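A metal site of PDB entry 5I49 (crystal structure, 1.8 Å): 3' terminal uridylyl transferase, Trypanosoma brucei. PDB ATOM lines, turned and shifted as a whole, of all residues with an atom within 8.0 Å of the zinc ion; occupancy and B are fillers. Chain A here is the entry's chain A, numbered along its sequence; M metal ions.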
ATOM      1  N   SER A   7       8.706 -25.913  -5.189  1.00  0.00           N
ATOM      2  CA  SER A   7       9.763 -25.737  -4.198  1.00  0.00           C
ATOM      3  C   SER A   7       9.380 -26.302  -2.835  1.00  0.00           C
ATOM      4  O   SER A   7       8.204 -26.340  -2.467  1.00  0.00           O
ATOM      5  CB  SER A   7      10.176 -24.274  -4.074  1.00  0.00           C
ATOM      6  OG  SER A   7       9.097 -23.484  -3.611  1.00  0.00           O
ATOM      7  N   CYS A   8      10.373 -26.760  -2.078  1.00  0.00           N
ATOM      8  CA  CYS A   8      10.131 -27.307  -0.750  1.00  0.00           C
ATOM      9  C   CYS A   8       9.927 -26.195   0.259  1.00  0.00           C
ATOM     10  O   CYS A   8      10.410 -25.078   0.062  1.00  0.00           O
ATOM     11  CB  CYS A   8      11.311 -28.178  -0.321  1.00  0.00           C
ATOM     12  SG  CYS A   8      11.046 -28.964   1.267  1.00  0.00           S
ATOM     13  N   ASP A   9       9.206 -26.493   1.347  1.00  0.00           N
ATOM     14  CA  ASP A   9       8.948 -25.477   2.374  1.00  0.00           C
ATOM     15  C   ASP A   9       9.725 -25.763   3.659  1.00  0.00           C
ATOM     16  O   ASP A   9       9.530 -25.077   4.668  1.00  0.00           O
ATOM     17  CB  ASP A   9       7.451 -25.427   2.696  1.00  0.00           C
ATOM     18  CG  ASP A   9       6.938 -26.723   3.294  1.00  0.00           C
ATOM     19  OD1 ASP A   9       7.523 -27.791   2.998  1.00  0.00           O
ATOM     20  OD2 ASP A   9       5.935 -26.692   4.034  1.00  0.00           O
ATOM     21  N   ALA A  10      10.594 -26.771   3.606  1.00  0.00           N
ATOM     22  CA  ALA A  10      11.331 -27.214   4.799  1.00  0.00           C
ATOM     23  C   ALA A  10      12.828 -26.996   4.650  1.00  0.00           C
ATOM     24  O   ALA A  10      13.596 -27.193   5.592  1.00  0.00           O
ATOM     25  CB  ALA A  10      11.065 -28.675   5.051  1.00  0.00           C
ATOM     26  N   CYS A  11      13.251 -26.620   3.446  1.00  0.00           N
ATOM     27  CA  CYS A  11      14.648 -26.294   3.195  1.00  0.00           C
ATOM     28  C   CYS A  11      14.710 -25.325   2.020  1.00  0.00           C
ATOM     29  O   CYS A  11      13.829 -25.340   1.160  1.00  0.00           O
ATOM     30  CB  CYS A  11      15.466 -27.572   2.950  1.00  0.00           C
ATOM     31  SG  CYS A  11      15.369 -28.275   1.303  1.00  0.00           S
ATOM     32  N   PRO A  12      15.738 -24.463   1.983  1.00  0.00           N
ATOM     33  CA  PRO A  12      15.714 -23.335   1.053  1.00  0.00           C
ATOM     34  C   PRO A  12      16.182 -23.660  -0.363  1.00  0.00           C
ATOM     35  O   PRO A  12      16.001 -22.832  -1.255  1.00  0.00           O
ATOM     36  CB  PRO A  12      16.692 -22.352   1.705  1.00  0.00           C
ATOM     37  CG  PRO A  12      17.698 -23.232   2.340  1.00  0.00           C
ATOM     38  CD  PRO A  12      16.950 -24.455   2.823  1.00  0.00           C
ATOM     39  N   HIS A  13      16.733 -24.858  -0.572  1.00  0.00           N
ATOM     40  CA  HIS A  13      17.492 -25.161  -1.779  1.00  0.00           C
ATOM     41  C   HIS A  13      16.917 -26.266  -2.674  1.00  0.00           C
ATOM     42  O   HIS A  13      17.624 -26.801  -3.540  1.00  0.00           O
ATOM     43  CB  HIS A  13      18.907 -25.574  -1.368  1.00  0.00           C
ATOM     44  CG  HIS A  13      18.949 -26.819  -0.527  1.00  0.00           C
ATOM     45  ND1 HIS A  13      19.112 -26.790   0.842  1.00  0.00           N
ATOM     46  CD2 HIS A  13      18.816 -28.124  -0.855  1.00  0.00           C
ATOM     47  CE1 HIS A  13      19.102 -28.029   1.315  1.00  0.00           C
ATOM     48  NE2 HIS A  13      18.919 -28.857   0.304  1.00  0.00           N
ATOM     49  N   ALA A  14      15.667 -26.623  -2.478  1.00  0.00           N
ATOM     50  CA  ALA A  14      15.098 -27.743  -3.218  1.00  0.00           C
ATOM     51  C   ALA A  14      13.977 -27.311  -4.153  1.00  0.00           C
ATOM     52  O   ALA A  14      12.890 -26.962  -3.707  1.00  0.00           O
ATOM     53  CB  ALA A  14      14.606 -28.822  -2.265  1.00  0.00           C
ATOM     54  N   VAL A  15      14.258 -27.337  -5.453  1.00  0.00           N
ATOM     55  CA  VAL A  15      13.260 -26.993  -6.463  1.00  0.00           C
ATOM     56  C   VAL A  15      13.169 -28.108  -7.510  1.00  0.00           C
ATOM     57  O   VAL A  15      14.169 -28.725  -7.873  1.00  0.00           O
ATOM     58  CB  VAL A  15      13.550 -25.630  -7.123  1.00  0.00           C
ATOM     59  CG1 VAL A  15      13.593 -24.536  -6.082  1.00  0.00           C
ATOM     60  CG2 VAL A  15      14.866 -25.678  -7.872  1.00  0.00           C
ATOM     61  N   PHE A  16      11.949 -28.372  -7.975  1.00  0.00           N
ATOM     62  CA  PHE A  16      11.730 -29.501  -8.877  1.00  0.00           C
ATOM     63  C   PHE A  16      10.821 -29.083 -10.023  1.00  0.00           C
ATOM     64  O   PHE A  16      10.193 -28.018  -9.972  1.00  0.00           O
ATOM     65  CB  PHE A  16      11.127 -30.664  -8.090  1.00  0.00           C
ATOM     66  CG  PHE A  16      11.908 -31.020  -6.863  1.00  0.00           C
ATOM     67  CD1 PHE A  16      12.933 -31.958  -6.930  1.00  0.00           C
ATOM     68  CD2 PHE A  16      11.629 -30.403  -5.647  1.00  0.00           C
ATOM     69  CE1 PHE A  16      13.657 -32.284  -5.790  1.00  0.00           C
ATOM     70  CE2 PHE A  16      12.356 -30.715  -4.510  1.00  0.00           C
ATOM     71  CZ  PHE A  16      13.381 -31.655  -4.587  1.00  0.00           C
ATOM     72  N   LEU A  22       8.697 -33.449  -5.916  1.00  0.00           N
ATOM     73  CA  LEU A  22       8.534 -32.628  -4.709  1.00  0.00           C
ATOM     74  C   LEU A  22       8.082 -33.488  -3.533  1.00  0.00           C
ATOM     75  O   LEU A  22       8.653 -33.400  -2.452  1.00  0.00           O
ATOM     76  CB  LEU A  22       7.527 -31.488  -4.945  1.00  0.00           C
ATOM     77  CG  LEU A  22       7.313 -30.558  -3.749  1.00  0.00           C
ATOM     78  CD1 LEU A  22       8.548 -29.728  -3.486  1.00  0.00           C
ATOM     79  CD2 LEU A  22       6.076 -29.675  -3.905  1.00  0.00           C
ATOM     80  N   HIS A  25      10.771 -35.865  -2.422  1.00  0.00           N
ATOM     81  CA  HIS A  25      11.731 -35.115  -1.623  1.00  0.00           C
ATOM     82  C   HIS A  25      11.231 -34.847  -0.196  1.00  0.00           C
ATOM     83  O   HIS A  25      12.004 -34.940   0.756  1.00  0.00           O
ATOM     84  CB  HIS A  25      12.052 -33.778  -2.279  1.00  0.00           C
ATOM     85  CG  HIS A  25      12.816 -32.862  -1.378  1.00  0.00           C
ATOM     86  ND1 HIS A  25      14.172 -32.963  -1.190  1.00  0.00           N
ATOM     87  CD2 HIS A  25      12.390 -31.859  -0.582  1.00  0.00           C
ATOM     88  CE1 HIS A  25      14.566 -32.031  -0.343  1.00  0.00           C
ATOM     89  NE2 HIS A  25      13.502 -31.365   0.062  1.00  0.00           N
ATOM     90  N   ALA A  26       9.962 -34.485  -0.048  1.00  0.00           N
ATOM     91  CA  ALA A  26       9.409 -34.248   1.283  1.00  0.00           C
ATOM     92  C   ALA A  26       9.512 -35.505   2.157  1.00  0.00           C
ATOM     93  O   ALA A  26       9.926 -35.439   3.314  1.00  0.00           O
ATOM     94  CB  ALA A  26       7.946 -33.767   1.216  1.00  0.00           C
ATOM     95  N   HIS A  29      13.610 -36.558   2.509  1.00  0.00           N
ATOM     96  CA  HIS A  29      14.494 -35.643   3.215  1.00  0.00           C
ATOM     97  C   HIS A  29      13.871 -34.979   4.454  1.00  0.00           C
ATOM     98  O   HIS A  29      14.582 -34.334   5.224  1.00  0.00           O
ATOM     99  CB  HIS A  29      15.053 -34.593   2.258  1.00  0.00           C
ATOM    100  CG  HIS A  29      15.998 -35.150   1.242  1.00  0.00           C
ATOM    101  ND1 HIS A  29      15.589 -35.923   0.180  1.00  0.00           N
ATOM    102  CD2 HIS A  29      17.344 -35.045   1.125  1.00  0.00           C
ATOM    103  CE1 HIS A  29      16.636 -36.268  -0.551  1.00  0.00           C
ATOM    104  NE2 HIS A  29      17.719 -35.749   0.007  1.00  0.00           N
ATOM    105  N   HIS A  30      12.563 -35.143   4.643  1.00  0.00           N
ATOM    106  CA  HIS A  30      11.897 -34.492   5.772  1.00  0.00           C
ATOM    107  C   HIS A  30      10.935 -35.379   6.537  1.00  0.00           C
ATOM    108  O   HIS A  30       9.939 -34.909   7.092  1.00  0.00           O
ATOM    109  CB  HIS A  30      11.172 -33.221   5.316  1.00  0.00           C
ATOM    110  CG  HIS A  30      12.092 -32.221   4.713  1.00  0.00           C
ATOM    111  ND1 HIS A  30      13.100 -31.614   5.427  1.00  0.00           N
ATOM    112  CD2 HIS A  30      12.194 -31.761   3.442  1.00  0.00           C
ATOM    113  CE1 HIS A  30      13.769 -30.801   4.637  1.00  0.00           C
ATOM    114  NE2 HIS A  30      13.241 -30.869   3.430  1.00  0.00           N
ATOM    115  N   LEU A  33       9.695 -34.308   9.849  1.00  0.00           N
ATOM    116  CA  LEU A  33       8.613 -33.323   9.917  1.00  0.00           C
ATOM    117  C   LEU A  33       7.248 -33.953   9.686  1.00  0.00           C
ATOM    118  O   LEU A  33       6.218 -33.354  10.002  1.00  0.00           O
ATOM    119  CB  LEU A  33       8.839 -32.225   8.880  1.00  0.00           C
ATOM    120  CG  LEU A  33      10.045 -31.326   9.099  1.00  0.00           C
ATOM    121  CD1 LEU A  33      10.076 -30.228   8.063  1.00  0.00           C
ATOM    122  CD2 LEU A  33      10.037 -30.732  10.492  1.00  0.00           C
ATOM    123  N   VAL A 481       4.632 -27.958   1.146  1.00  0.00           N
ATOM    124  CA  VAL A 481       4.546 -29.413   0.958  1.00  0.00           C
ATOM    125  C   VAL A 481       4.654 -30.255   2.240  1.00  0.00           C
ATOM    126  O   VAL A 481       3.830 -31.150   2.456  1.00  0.00           O
ATOM    127  CB  VAL A 481       5.464 -29.935  -0.166  1.00  0.00           C
ATOM    128  CG1 VAL A 481       6.962 -29.749   0.170  1.00  0.00           C
ATOM    129  CG2 VAL A 481       5.170 -31.407  -0.452  1.00  0.00           C
ATOM    130  N   THR A 482       5.651 -29.999   3.094  1.00  0.00           N
ATOM    131  CA  THR A 482       5.770 -30.795   4.317  1.00  0.00           C
ATOM    132  C   THR A 482       4.593 -30.541   5.249  1.00  0.00           C
ATOM    133  O   THR A 482       4.066 -31.474   5.858  1.00  0.00           O
ATOM    134  CB  THR A 482       7.117 -30.574   5.064  1.00  0.00           C
ATOM    135  OG1 THR A 482       7.238 -29.202   5.461  1.00  0.00           O
ATOM    136  CG2 THR A 482       8.273 -30.939   4.153  1.00  0.00           C
HETATM  137 ZN    ZN M   1      13.333 -29.750   1.503  1.00  0.00          ZN
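The backbone NH of Cys 8 sits at hydrogen-bond distance from the backbone carbonyl oxygen of Ala 14 (3.0 Å). The side-chain sulfur (SG) of Cys 8 lies close to the backbone NH (N) of Ala 10. SG of Cys 11 sits close to NE2 of His 13 (3.7 Å).
The nearest printed residue that does not touch the zinc ion is Ala 14 (4.1 Å).
The zinc ion is bound by a ring nitrogen (NE2) of His 25 (2.2 Å), a ring nitrogen (NE2) of His 30 (2.2 Å), the side-chain sulfur of Cys 8 (2.4 Å) and the side-chain sulfur of Cys 11 (2.5 Å).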
